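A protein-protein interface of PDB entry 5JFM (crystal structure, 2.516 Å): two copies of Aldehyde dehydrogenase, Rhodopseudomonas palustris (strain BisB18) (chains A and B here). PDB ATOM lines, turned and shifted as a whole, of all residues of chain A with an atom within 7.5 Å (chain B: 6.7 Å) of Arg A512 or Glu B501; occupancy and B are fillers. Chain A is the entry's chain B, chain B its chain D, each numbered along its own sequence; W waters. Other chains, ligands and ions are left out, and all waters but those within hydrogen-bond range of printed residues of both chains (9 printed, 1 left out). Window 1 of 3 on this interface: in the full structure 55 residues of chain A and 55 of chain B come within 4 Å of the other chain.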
ATOM      1  N   ASP A 172      -2.442  36.415  -3.264  1.00  0.00           N
ATOM      2  CA  ASP A 172      -1.254  35.875  -2.604  1.00  0.00           C
ATOM      3  C   ASP A 172      -0.203  35.491  -3.635  1.00  0.00           C
ATOM      4  O   ASP A 172      -0.514  34.891  -4.669  1.00  0.00           O
ATOM      5  CB  ASP A 172      -1.598  34.652  -1.758  1.00  0.00           C
ATOM      6  CG  ASP A 172      -2.400  34.999  -0.536  1.00  0.00           C
ATOM      7  OD1 ASP A 172      -2.273  36.152  -0.079  1.00  0.00           O
ATOM      8  OD2 ASP A 172      -3.151  34.127  -0.033  1.00  0.00           O
ATOM      9  N   VAL A 183      -2.269  33.167  -6.065  1.00  0.00           N
ATOM     10  CA  VAL A 183      -3.521  32.664  -5.506  1.00  0.00           C
ATOM     11  C   VAL A 183      -4.549  33.791  -5.561  1.00  0.00           C
ATOM     12  O   VAL A 183      -4.338  34.852  -4.958  1.00  0.00           O
ATOM     13  CB  VAL A 183      -3.337  32.148  -4.064  1.00  0.00           C
ATOM     14  CG1 VAL A 183      -4.637  31.580  -3.512  1.00  0.00           C
ATOM     15  CG2 VAL A 183      -2.260  31.076  -4.019  1.00  0.00           C
ATOM     16  N   GLU A 184      -5.654  33.564  -6.278  1.00  0.00           N
ATOM     17  CA  GLU A 184      -6.694  34.571  -6.505  1.00  0.00           C
ATOM     18  C   GLU A 184      -8.060  34.085  -6.024  1.00  0.00           C
ATOM     19  O   GLU A 184      -8.301  32.888  -5.856  1.00  0.00           O
ATOM     20  CB  GLU A 184      -6.812  34.933  -7.992  1.00  0.00           C
ATOM     21  CG  GLU A 184      -5.500  35.298  -8.684  1.00  0.00           C
ATOM     22  CD  GLU A 184      -5.165  36.764  -8.540  1.00  0.00           C
ATOM     23  OE1 GLU A 184      -5.759  37.440  -7.664  1.00  0.00           O
ATOM     24  OE2 GLU A 184      -4.312  37.243  -9.318  1.00  0.00           O
ATOM     25  N   TYR A 185      -8.967  35.037  -5.833  1.00  0.00           N
ATOM     26  CA  TYR A 185     -10.357  34.768  -5.475  1.00  0.00           C
ATOM     27  C   TYR A 185     -11.239  34.989  -6.702  1.00  0.00           C
ATOM     28  O   TYR A 185     -11.412  36.126  -7.146  1.00  0.00           O
ATOM     29  CB  TYR A 185     -10.805  35.675  -4.340  1.00  0.00           C
ATOM     30  CG  TYR A 185     -10.133  35.425  -3.023  1.00  0.00           C
ATOM     31  CD1 TYR A 185     -10.579  34.419  -2.181  1.00  0.00           C
ATOM     32  CD2 TYR A 185      -9.065  36.215  -2.602  1.00  0.00           C
ATOM     33  CE1 TYR A 185      -9.980  34.195  -0.958  1.00  0.00           C
ATOM     34  CE2 TYR A 185      -8.458  36.005  -1.378  1.00  0.00           C
ATOM     35  CZ  TYR A 185      -8.921  34.985  -0.555  1.00  0.00           C
ATOM     36  OH  TYR A 185      -8.331  34.740   0.669  1.00  0.00           O
ATOM     37  N   SER A 186     -11.824  33.916  -7.220  1.00  0.00           N
ATOM     38  CA  SER A 186     -12.566  33.925  -8.469  1.00  0.00           C
ATOM     39  C   SER A 186     -14.032  33.568  -8.231  1.00  0.00           C
ATOM     40  O   SER A 186     -14.382  33.053  -7.160  1.00  0.00           O
ATOM     41  CB  SER A 186     -11.917  32.950  -9.462  1.00  0.00           C
ATOM     42  OG  SER A 186     -10.807  33.572 -10.083  1.00  0.00           O
ATOM     43  N   PRO A 187     -14.916  33.827  -9.202  1.00  0.00           N
ATOM     44  CA  PRO A 187     -16.358  33.673  -8.948  1.00  0.00           C
ATOM     45  C   PRO A 187     -16.804  32.225  -8.794  1.00  0.00           C
ATOM     46  O   PRO A 187     -16.288  31.316  -9.447  1.00  0.00           O
ATOM     47  CB  PRO A 187     -17.006  34.295 -10.192  1.00  0.00           C
ATOM     48  CG  PRO A 187     -15.949  35.139 -10.818  1.00  0.00           C
ATOM     49  CD  PRO A 187     -14.662  34.455 -10.511  1.00  0.00           C
ATOM     50  N   PHE A 188     -17.811  32.038  -7.935  1.00  0.00           N
ATOM     51  CA  PHE A 188     -18.518  30.764  -7.821  1.00  0.00           C
ATOM     52  C   PHE A 188     -19.508  30.553  -8.963  1.00  0.00           C
ATOM     53  O   PHE A 188     -19.584  29.459  -9.533  1.00  0.00           O
ATOM     54  CB  PHE A 188     -19.257  30.692  -6.481  1.00  0.00           C
ATOM     55  CG  PHE A 188     -18.583  29.820  -5.476  1.00  0.00           C
ATOM     56  CD1 PHE A 188     -18.769  28.452  -5.498  1.00  0.00           C
ATOM     57  CD2 PHE A 188     -17.737  30.362  -4.525  1.00  0.00           C
ATOM     58  CE1 PHE A 188     -18.139  27.645  -4.580  1.00  0.00           C
ATOM     59  CE2 PHE A 188     -17.106  29.564  -3.609  1.00  0.00           C
ATOM     60  CZ  PHE A 188     -17.307  28.199  -3.636  1.00  0.00           C
ATOM     61  N   LYS A 292     -22.451  23.583  -1.836  1.00  0.00           N
ATOM     62  CA  LYS A 292     -21.753  24.487  -0.942  1.00  0.00           C
ATOM     63  C   LYS A 292     -22.748  25.444  -0.300  1.00  0.00           C
ATOM     64  O   LYS A 292     -23.555  26.081  -0.986  1.00  0.00           O
ATOM     65  CB  LYS A 292     -20.686  25.250  -1.731  1.00  0.00           C
ATOM     66  CG  LYS A 292     -20.090  26.457  -1.013  1.00  0.00           C
ATOM     67  CD  LYS A 292     -19.103  26.051   0.073  1.00  0.00           C
ATOM     68  CE  LYS A 292     -18.257  27.248   0.520  1.00  0.00           C
ATOM     69  NZ  LYS A 292     -17.374  26.862   1.638  1.00  0.00           N
ATOM     70  N   THR A 499     -20.631  27.178   9.670  1.00  0.00           N
ATOM     71  CA  THR A 499     -19.678  26.949   8.592  1.00  0.00           C
ATOM     72  C   THR A 499     -18.381  27.731   8.761  1.00  0.00           C
ATOM     73  O   THR A 499     -17.472  27.578   7.938  1.00  0.00           O
ATOM     74  CB  THR A 499     -20.328  27.266   7.234  1.00  0.00           C
ATOM     75  OG1 THR A 499     -20.835  28.605   7.232  1.00  0.00           O
ATOM     76  CG2 THR A 499     -21.487  26.300   6.954  1.00  0.00           C
ATOM     77  N   GLU A 501     -17.030  30.790   8.473  1.00  0.00           N
ATOM     78  CA  GLU A 501     -16.420  31.837   7.663  1.00  0.00           C
ATOM     79  C   GLU A 501     -16.228  33.139   8.420  1.00  0.00           C
ATOM     80  O   GLU A 501     -15.471  33.997   7.954  1.00  0.00           O
ATOM     81  CB  GLU A 501     -17.261  32.131   6.414  1.00  0.00           C
ATOM     82  CG  GLU A 501     -17.193  31.084   5.343  1.00  0.00           C
ATOM     83  CD  GLU A 501     -18.048  29.880   5.668  1.00  0.00           C
ATOM     84  OE1 GLU A 501     -18.813  29.942   6.658  1.00  0.00           O
ATOM     85  OE2 GLU A 501     -17.932  28.863   4.948  1.00  0.00           O
ATOM     86  N   LYS A 507     -14.635  37.861  -0.235  1.00  0.00           N
ATOM     87  CA  LYS A 507     -13.800  36.661  -0.138  1.00  0.00           C
ATOM     88  C   LYS A 507     -14.619  35.408   0.141  1.00  0.00           C
ATOM     89  O   LYS A 507     -14.312  34.325  -0.380  1.00  0.00           O
ATOM     90  CB  LYS A 507     -12.778  36.831   0.987  1.00  0.00           C
ATOM     91  CG  LYS A 507     -11.373  37.200   0.589  1.00  0.00           C
ATOM     92  CD  LYS A 507     -10.431  37.031   1.796  1.00  0.00           C
ATOM     93  CE  LYS A 507     -10.439  38.239   2.734  1.00  0.00           C
ATOM     94  NZ  LYS A 507      -9.633  39.381   2.169  1.00  0.00           N
ATOM     95  N   ALA A 510     -16.136  33.451  -3.028  1.00  0.00           N
ATOM     96  CA  ALA A 510     -15.193  33.210  -4.102  1.00  0.00           C
ATOM     97  C   ALA A 510     -14.617  31.808  -3.980  1.00  0.00           C
ATOM     98  O   ALA A 510     -14.555  31.239  -2.886  1.00  0.00           O
ATOM     99  CB  ALA A 510     -14.052  34.254  -4.078  1.00  0.00           C
ATOM    100  N   ARG A 511     -14.201  31.259  -5.120  1.00  0.00           N
ATOM    101  CA  ARG A 511     -13.368  30.059  -5.173  1.00  0.00           C
ATOM    102  C   ARG A 511     -11.902  30.463  -5.156  1.00  0.00           C
ATOM    103  O   ARG A 511     -11.496  31.384  -5.867  1.00  0.00           O
ATOM    104  CB  ARG A 511     -13.619  29.256  -6.452  1.00  0.00           C
ATOM    105  CG  ARG A 511     -15.054  29.015  -6.805  1.00  0.00           C
ATOM    106  CD  ARG A 511     -15.177  28.439  -8.209  1.00  0.00           C
ATOM    107  NE  ARG A 511     -14.578  27.114  -8.297  1.00  0.00           N
ATOM    108  CZ  ARG A 511     -13.559  26.804  -9.089  1.00  0.00           C
ATOM    109  NH1 ARG A 511     -13.031  27.726  -9.888  1.00  0.00           N
ATOM    110  NH2 ARG A 511     -13.078  25.566  -9.095  1.00  0.00           N
ATOM    111  N   ARG A 512     -11.099  29.765  -4.364  1.00  0.00           N
ATOM    112  CA  ARG A 512      -9.670  30.055  -4.291  1.00  0.00           C
ATOM    113  C   ARG A 512      -8.937  29.275  -5.383  1.00  0.00           C
ATOM    114  O   ARG A 512      -8.995  28.041  -5.416  1.00  0.00           O
ATOM    115  CB  ARG A 512      -9.123  29.723  -2.902  1.00  0.00           C
ATOM    116  CG  ARG A 512      -7.635  30.011  -2.747  1.00  0.00           C
ATOM    117  CD  ARG A 512      -7.163  30.106  -1.287  1.00  0.00           C
ATOM    118  NE  ARG A 512      -7.059  28.798  -0.650  1.00  0.00           N
ATOM    119  CZ  ARG A 512      -6.530  28.585   0.550  1.00  0.00           C
ATOM    120  NH1 ARG A 512      -6.036  29.593   1.263  1.00  0.00           N
ATOM    121  NH2 ARG A 512      -6.492  27.358   1.041  1.00  0.00           N
ATOM    122  N   ARG A 513      -8.257  29.993  -6.278  1.00  0.00           N
ATOM    123  CA  ARG A 513      -7.566  29.400  -7.421  1.00  0.00           C
ATOM    124  C   ARG A 513      -6.063  29.654  -7.339  1.00  0.00           C
ATOM    125  O   ARG A 513      -5.621  30.717  -6.887  1.00  0.00           O
ATOM    126  CB  ARG A 513      -8.105  29.932  -8.760  1.00  0.00           C
ATOM    127  CG  ARG A 513      -9.499  29.420  -9.082  1.00  0.00           C
ATOM    128  CD  ARG A 513      -9.879  29.657 -10.532  1.00  0.00           C
ATOM    129  NE  ARG A 513      -9.179  30.809 -11.075  1.00  0.00           N
ATOM    130  CZ  ARG A 513      -8.353  30.758 -12.107  1.00  0.00           C
ATOM    131  NH1 ARG A 513      -8.130  29.612 -12.737  1.00  0.00           N
ATOM    132  NH2 ARG A 513      -7.747  31.858 -12.511  1.00  0.00           N
ATOM    133  N   LYS A 514      -5.289  28.665  -7.800  1.00  0.00           N
ATOM    134  CA  LYS A 514      -3.835  28.644  -7.695  1.00  0.00           C
ATOM    135  C   LYS A 514      -3.237  28.506  -9.088  1.00  0.00           C
ATOM    136  O   LYS A 514      -3.547  27.552  -9.812  1.00  0.00           O
ATOM    137  CB  LYS A 514      -3.378  27.494  -6.792  1.00  0.00           C
ATOM    138  CG  LYS A 514      -1.873  27.270  -6.697  1.00  0.00           C
ATOM    139  CD  LYS A 514      -1.578  26.101  -5.765  1.00  0.00           C
ATOM    140  CE  LYS A 514      -0.085  25.791  -5.680  1.00  0.00           C
ATOM    141  NZ  LYS A 514       0.221  24.701  -4.704  1.00  0.00           N
ATOM    142  N   MET B 273     -17.530  18.925  11.524  1.00  0.00           N
ATOM    143  CA  MET B 273     -17.124  19.185  10.149  1.00  0.00           C
ATOM    144  C   MET B 273     -16.752  17.867   9.482  1.00  0.00           C
ATOM    145  O   MET B 273     -16.058  17.037  10.082  1.00  0.00           O
ATOM    146  CB  MET B 273     -15.930  20.154  10.075  1.00  0.00           C
ATOM    147  CG  MET B 273     -15.345  20.325   8.650  1.00  0.00           C
ATOM    148  SD  MET B 273     -13.819  21.301   8.547  1.00  0.00           S
ATOM    149  CE  MET B 273     -14.403  22.914   8.039  1.00  0.00           C
ATOM    150  N   LYS B 292     -21.237  21.333   8.205  1.00  0.00           N
ATOM    151  CA  LYS B 292     -20.173  21.938   7.416  1.00  0.00           C
ATOM    152  C   LYS B 292     -19.350  20.853   6.729  1.00  0.00           C
ATOM    153  O   LYS B 292     -18.886  19.904   7.371  1.00  0.00           O
ATOM    154  CB  LYS B 292     -19.292  22.796   8.319  1.00  0.00           C
ATOM    155  CG  LYS B 292     -17.963  23.239   7.713  1.00  0.00           C
ATOM    156  CD  LYS B 292     -18.142  24.296   6.635  1.00  0.00           C
ATOM    157  CE  LYS B 292     -16.810  24.951   6.306  1.00  0.00           C
ATOM    158  NZ  LYS B 292     -16.960  26.029   5.299  1.00  0.00           N
ATOM    159  N   ALA B 293     -19.168  20.979   5.419  1.00  0.00           N
ATOM    160  CA  ALA B 293     -18.435  19.963   4.686  1.00  0.00           C
ATOM    161  C   ALA B 293     -17.483  20.602   3.688  1.00  0.00           C
ATOM    162  O   ALA B 293     -17.817  21.598   3.041  1.00  0.00           O
ATOM    163  CB  ALA B 293     -19.385  19.001   3.957  1.00  0.00           C
ATOM    164  N   ILE B 294     -16.294  20.014   3.571  1.00  0.00           N
ATOM    165  CA  ILE B 294     -15.373  20.289   2.477  1.00  0.00           C
ATOM    166  C   ILE B 294     -15.359  19.064   1.573  1.00  0.00           C
ATOM    167  O   ILE B 294     -15.321  17.927   2.060  1.00  0.00           O
ATOM    168  CB  ILE B 294     -13.962  20.631   3.002  1.00  0.00           C
ATOM    169  CG1 ILE B 294     -14.022  21.908   3.851  1.00  0.00           C
ATOM    170  CG2 ILE B 294     -12.965  20.767   1.852  1.00  0.00           C
ATOM    171  CD1 ILE B 294     -12.688  22.415   4.336  1.00  0.00           C
ATOM    172  N   GLY B 295     -15.420  19.289   0.258  1.00  0.00           N
ATOM    173  CA  GLY B 295     -15.414  18.181  -0.684  1.00  0.00           C
ATOM    174  C   GLY B 295     -14.383  18.251  -1.798  1.00  0.00           C
ATOM    175  O   GLY B 295     -14.207  19.298  -2.430  1.00  0.00           O
ATOM    176  N   THR B 470      -9.670  27.092 -13.410  1.00  0.00           N
ATOM    177  CA  THR B 470      -9.425  25.864 -12.666  1.00  0.00           C
ATOM    178  C   THR B 470      -8.822  26.159 -11.290  1.00  0.00           C
ATOM    179  O   THR B 470      -8.111  27.147 -11.095  1.00  0.00           O
ATOM    180  CB  THR B 470      -8.505  24.924 -13.453  1.00  0.00           C
ATOM    181  OG1 THR B 470      -7.329  25.633 -13.871  1.00  0.00           O
ATOM    182  CG2 THR B 470      -9.230  24.360 -14.687  1.00  0.00           C
ATOM    183  N   THR B 471      -9.138  25.287 -10.328  1.00  0.00           N
ATOM    184  CA  THR B 471      -8.572  25.405  -8.985  1.00  0.00           C
ATOM    185  C   THR B 471      -7.044  25.367  -9.021  1.00  0.00           C
ATOM    186  O   THR B 471      -6.376  26.052  -8.235  1.00  0.00           O
ATOM    187  CB  THR B 471      -9.128  24.283  -8.097  1.00  0.00           C
ATOM    188  OG1 THR B 471     -10.563  24.331  -8.120  1.00  0.00           O
ATOM    189  CG2 THR B 471      -8.651  24.418  -6.656  1.00  0.00           C
ATOM    190  N   ILE B 472      -6.476  24.578  -9.927  1.00  0.00           N
ATOM    191  CA  ILE B 472      -5.039  24.526 -10.135  1.00  0.00           C
ATOM    192  C   ILE B 472      -4.778  24.781 -11.612  1.00  0.00           C
ATOM    193  O   ILE B 472      -5.516  24.300 -12.479  1.00  0.00           O
ATOM    194  CB  ILE B 472      -4.433  23.178  -9.689  1.00  0.00           C
ATOM    195  CG1 ILE B 472      -4.694  22.946  -8.203  1.00  0.00           C
ATOM    196  CG2 ILE B 472      -2.916  23.132  -9.951  1.00  0.00           C
ATOM    197  CD1 ILE B 472      -4.106  21.680  -7.715  1.00  0.00           C
ATOM    198  N   TYR B 490       2.611  25.567  -0.850  1.00  0.00           N
ATOM    199  CA  TYR B 490       2.571  24.397   0.009  1.00  0.00           C
ATOM    200  C   TYR B 490       1.893  23.241  -0.719  1.00  0.00           C
ATOM    201  O   TYR B 490       1.361  23.394  -1.820  1.00  0.00           O
ATOM    202  CB  TYR B 490       1.858  24.718   1.320  1.00  0.00           C
ATOM    203  CG  TYR B 490       0.443  25.216   1.157  1.00  0.00           C
ATOM    204  CD1 TYR B 490       0.174  26.566   0.971  1.00  0.00           C
ATOM    205  CD2 TYR B 490      -0.628  24.333   1.203  1.00  0.00           C
ATOM    206  CE1 TYR B 490      -1.121  27.019   0.832  1.00  0.00           C
ATOM    207  CE2 TYR B 490      -1.914  24.776   1.060  1.00  0.00           C
ATOM    208  CZ  TYR B 490      -2.160  26.110   0.872  1.00  0.00           C
ATOM    209  OH  TYR B 490      -3.460  26.531   0.730  1.00  0.00           O
ATOM    210  N   ILE B 495      -7.749  18.686  -2.336  1.00  0.00           N
ATOM    211  CA  ILE B 495      -7.994  19.831  -3.198  1.00  0.00           C
ATOM    212  C   ILE B 495      -9.501  19.966  -3.314  1.00  0.00           C
ATOM    213  O   ILE B 495     -10.165  19.097  -3.891  1.00  0.00           O
ATOM    214  CB  ILE B 495      -7.335  19.636  -4.569  1.00  0.00           C
ATOM    215  CG1 ILE B 495      -5.854  19.302  -4.385  1.00  0.00           C
ATOM    216  CG2 ILE B 495      -7.542  20.848  -5.460  1.00  0.00           C
ATOM    217  CD1 ILE B 495      -5.284  18.554  -5.535  1.00  0.00           C
ATOM    218  N   ALA B 496     -10.049  21.033  -2.741  1.00  0.00           N
ATOM    219  CA  ALA B 496     -11.492  21.202  -2.754  1.00  0.00           C
ATOM    220  C   ALA B 496     -11.981  21.391  -4.180  1.00  0.00           C
ATOM    221  O   ALA B 496     -11.300  21.990  -5.017  1.00  0.00           O
ATOM    222  CB  ALA B 496     -11.909  22.397  -1.896  1.00  0.00           C
ATOM    223  N   GLY B 497     -13.163  20.860  -4.458  1.00  0.00           N
ATOM    224  CA  GLY B 497     -13.785  21.052  -5.738  1.00  0.00           C
ATOM    225  C   GLY B 497     -14.944  22.007  -5.618  1.00  0.00           C
ATOM    226  O   GLY B 497     -14.821  23.217  -5.851  1.00  0.00           O
ATOM    227  N   PRO B 498     -16.104  21.475  -5.231  1.00  0.00           N
ATOM    228  CA  PRO B 498     -17.309  22.305  -5.184  1.00  0.00           C
ATOM    229  C   PRO B 498     -17.354  23.269  -4.007  1.00  0.00           C
ATOM    230  O   PRO B 498     -18.099  24.258  -4.073  1.00  0.00           O
ATOM    231  CB  PRO B 498     -18.442  21.272  -5.107  1.00  0.00           C
ATOM    232  CG  PRO B 498     -17.817  20.077  -4.497  1.00  0.00           C
ATOM    233  CD  PRO B 498     -16.396  20.056  -4.984  1.00  0.00           C
ATOM    234  N   THR B 499     -16.605  23.032  -2.933  1.00  0.00           N
ATOM    235  CA  THR B 499     -16.762  23.900  -1.772  1.00  0.00           C
ATOM    236  C   THR B 499     -15.820  25.099  -1.773  1.00  0.00           C
ATOM    237  O   THR B 499     -15.954  25.968  -0.908  1.00  0.00           O
ATOM    238  CB  THR B 499     -16.595  23.101  -0.476  1.00  0.00           C
ATOM    239  OG1 THR B 499     -15.448  22.246  -0.581  1.00  0.00           O
ATOM    240  CG2 THR B 499     -17.844  22.270  -0.200  1.00  0.00           C
ATOM    241  N   GLY B 500     -14.874  25.175  -2.703  1.00  0.00           N
ATOM    242  CA  GLY B 500     -14.194  26.425  -2.965  1.00  0.00           C
ATOM    243  C   GLY B 500     -12.918  26.701  -2.197  1.00  0.00           C
ATOM    244  O   GLY B 500     -12.256  27.704  -2.491  1.00  0.00           O
ATOM    245  N   GLU B 501     -12.533  25.853  -1.236  1.00  0.00           N
ATOM    246  CA  GLU B 501     -11.396  26.200  -0.386  1.00  0.00           C
ATOM    247  C   GLU B 501     -10.047  26.072  -1.090  1.00  0.00           C
ATOM    248  O   GLU B 501      -9.027  26.433  -0.495  1.00  0.00           O
ATOM    249  CB  GLU B 501     -11.370  25.336   0.872  1.00  0.00           C
ATOM    250  CG  GLU B 501     -12.532  25.541   1.819  1.00  0.00           C
ATOM    251  CD  GLU B 501     -13.781  24.780   1.385  1.00  0.00           C
ATOM    252  OE1 GLU B 501     -13.764  24.151   0.284  1.00  0.00           O
ATOM    253  OE2 GLU B 501     -14.779  24.834   2.146  1.00  0.00           O
ATOM    254  N   GLY B 502     -10.006  25.568  -2.320  1.00  0.00           N
ATOM    255  CA  GLY B 502      -8.717  25.395  -2.970  1.00  0.00           C
ATOM    256  C   GLY B 502      -7.909  24.302  -2.292  1.00  0.00           C
ATOM    257  O   GLY B 502      -8.451  23.291  -1.829  1.00  0.00           O
ATOM    258  N   LEU B 503      -6.595  24.516  -2.216  1.00  0.00           N
ATOM    259  CA  LEU B 503      -5.686  23.559  -1.587  1.00  0.00           C
ATOM    260  C   LEU B 503      -5.822  23.663  -0.073  1.00  0.00           C
ATOM    261  O   LEU B 503      -5.336  24.624   0.531  1.00  0.00           O
ATOM    262  CB  LEU B 503      -4.247  23.817  -2.033  1.00  0.00           C
ATOM    263  CG  LEU B 503      -3.897  23.376  -3.466  1.00  0.00           C
ATOM    264  CD1 LEU B 503      -4.419  24.372  -4.519  1.00  0.00           C
ATOM    265  CD2 LEU B 503      -2.401  23.100  -3.648  1.00  0.00           C
ATOM    266  N   THR B 504      -6.469  22.677   0.551  1.00  0.00           N
ATOM    267  CA  THR B 504      -6.744  22.800   1.976  1.00  0.00           C
ATOM    268  C   THR B 504      -5.449  22.809   2.777  1.00  0.00           C
ATOM    269  O   THR B 504      -4.429  22.259   2.359  1.00  0.00           O
ATOM    270  CB  THR B 504      -7.647  21.670   2.474  1.00  0.00           C
ATOM    271  OG1 THR B 504      -7.033  20.404   2.218  1.00  0.00           O
ATOM    272  CG2 THR B 504      -9.005  21.731   1.810  1.00  0.00           C
ATOM    273  N   SER B 505      -5.499  23.479   3.922  1.00  0.00           N
ATOM    274  CA  SER B 505      -4.437  23.495   4.925  1.00  0.00           C
ATOM    275  C   SER B 505      -5.098  23.759   6.278  1.00  0.00           C
ATOM    276  O   SER B 505      -6.326  23.693   6.400  1.00  0.00           O
ATOM    277  CB  SER B 505      -3.348  24.531   4.571  1.00  0.00           C
ATOM    278  OG  SER B 505      -3.840  25.863   4.585  1.00  0.00           O
ATOM    279  N   LYS B 507      -5.717  26.466   7.992  1.00  0.00           N
ATOM    280  CA  LYS B 507      -6.752  27.497   7.896  1.00  0.00           C
ATOM    281  C   LYS B 507      -8.119  26.907   7.566  1.00  0.00           C
ATOM    282  O   LYS B 507      -9.138  27.336   8.121  1.00  0.00           O
ATOM    283  CB  LYS B 507      -6.401  28.524   6.809  1.00  0.00           C
ATOM    284  CG  LYS B 507      -5.260  29.464   7.094  1.00  0.00           C
ATOM    285  CD  LYS B 507      -5.082  30.463   5.932  1.00  0.00           C
ATOM    286  CE  LYS B 507      -3.855  31.354   6.165  1.00  0.00           C
ATOM    287  NZ  LYS B 507      -3.869  32.605   5.347  1.00  0.00           N
ATOM    288  N   SER B 508      -8.162  25.953   6.630  1.00  0.00           N
ATOM    289  CA  SER B 508      -9.430  25.424   6.144  1.00  0.00           C
ATOM    290  C   SER B 508     -10.183  24.645   7.211  1.00  0.00           C
ATOM    291  O   SER B 508     -11.380  24.394   7.046  1.00  0.00           O
ATOM    292  CB  SER B 508      -9.207  24.517   4.930  1.00  0.00           C
ATOM    293  OG  SER B 508      -8.251  25.057   4.030  1.00  0.00           O
HETATM  294  O   HOH W   1      -6.588  26.648  -5.457  1.00  0.00           O
HETATM  295  O   HOH W   2     -14.825  27.166   3.908  1.00  0.00           O
HETATM  296  O   HOH W   3     -15.005  28.481   6.684  1.00  0.00           O
HETATM  297  O   HOH W   4       0.379  25.949  -2.553  1.00  0.00           O
HETATM  298  O   HOH W   5     -15.106  28.343  -0.034  1.00  0.00           O
HETATM  299  O   HOH W   6     -19.391  26.471   3.455  1.00  0.00           O
HETATM  300  O   HOH W   7     -11.249  26.798  -6.371  1.00  0.00           O
HETATM  301  O   HOH W   8      -5.708  26.958  -2.808  1.00  0.00           O
HETATM  302  O   HOH W   9     -17.723  24.400   3.134  1.00  0.00           O
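The backbone carbonyl oxygen (O) of Thr B499 sits close to the side-chain amino group (NZ) of Lys A292.
The side-chain amino group of Lys A292 is in salt-bridge range of the side-chain carboxylate of Glu B501, 3.3 Å away.
The side-chain amino group of Lys B292 sits at hydrogen-bond distance from the backbone carbonyl oxygen of Thr A499 (3.1 Å).
The side-chain amino group of Lys B292 lies within salt-bridge range of the side-chain carboxylate of Glu A501.
The guanidinium group (NH2) of Arg A511 lies within hydrogen-bond range of the side-chain hydroxyl (OG1) of Thr B471 (3.0 Å).
The guanidinium group of Arg A512 lies within hydrogen-bond range of the side-chain hydroxyl of Tyr B490, at 3.2 Å.
The backbone NH of Arg A512 sits at hydrogen-bond distance from the backbone carbonyl oxygen of Gly B500 (3.0 Å).
The backbone carbonyl oxygen (O) of Glu B501 lies within hydrogen-bond range of the guanidinium group (NE) of Arg A512, 3.1 Å away.
NH2 of Arg A512 lies within hydrogen-bond range of O of Leu B503 (3.0 Å).
The guanidinium group (NH1) of Arg A513 sits at hydrogen-bond distance from the backbone carbonyl oxygen (O) of Thr B470.
O of Thr B471 lies within hydrogen-bond range of N of Lys A514.
The backbone carbonyl oxygen (O) of Tyr B490 is in hydrogen-bond range of the side-chain amino group (NZ) of Lys A514, at 3.4 Å.
The backbone NH (N) of Arg A511 sits at hydrogen-bond distance from the backbone carbonyl oxygen (O) of Ser A186 (2.7 Å).
The backbone NH (N) of Ala B496 sits at hydrogen-bond distance from the backbone carbonyl oxygen (O) of Gly B502 (2.9 Å).
Among the printed residues, merely in contact across the chains: Phe A188 with Pro B498, Phe A188 with Thr B499, Phe A188 with Gly B500, Lys A292 with Lys B292, Lys A292 with Pro B498, Arg A511 with Gly B500, Arg A512 with Thr B471, Arg A512 with Gly B502, Arg A513 with Thr B471, Lys A514 with Ile B472 and Lys A514 with Leu B503.
Ala A510 touches none of the printed residues of chain B.
Printed residues of chain B within 4 Å of Arg A512: Thr B471, Tyr B490, Gly B500, Glu B501, Gly B502 and Leu B503.
Of the printed residues of chain A, Glu B501 touches Lys A292 and Arg A512.
The nearest printed residue of chain A that does not touch Glu B501 is Arg A511 (5.8 Å).
The nearest printed residue of chain B that does not touch Arg A511 is Gly B497 (4.4 Å).
Printed residues of chain A that touch a printed residue of chain B: Phe A188, Lys A292, Thr A499, Glu A501, Arg A511, Arg A512, Arg A513 and Lys A514.
Hydrophobic or aromatic side chains of chain A within 4 Å of the printed part of chain B: Phe A188.
Along chain A the printed residues that touch a printed residue of chain B span positions 188 to 514.
Along chain B the printed residues that touch a printed residue of chain A span positions 292 to 503.
Among the printed residues, 23 pairs touch across the chains.
Among the printed residues, Asp or Glu carboxylates within 4 Å of a Lys or Arg side-chain nitrogen of the other chain: Lys A292 with Glu B501 (3.3 Å) and Glu A501 with Lys B292 (3.0 Å).
Lys A292 touches its own counterpart, Lys B292.
Lys A292 touches Thr B499, and with the chains exchanged Thr A499 touches Lys B292.
Lys A292 touches Glu B501, and with the chains exchanged Glu A501 touches Lys B292.
4 positions are printed for both chains.
Water W7 bridges O of Arg A512 and OG1 of Thr B471.
Water W1 lies within hydrogen-bond range of the backbone carbonyl oxygen of Arg A512 (2.8 Å), the backbone carbonyl oxygen of Thr B471 (2.8 Å) and the backbone NH of Lys A514 (3.4 Å).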
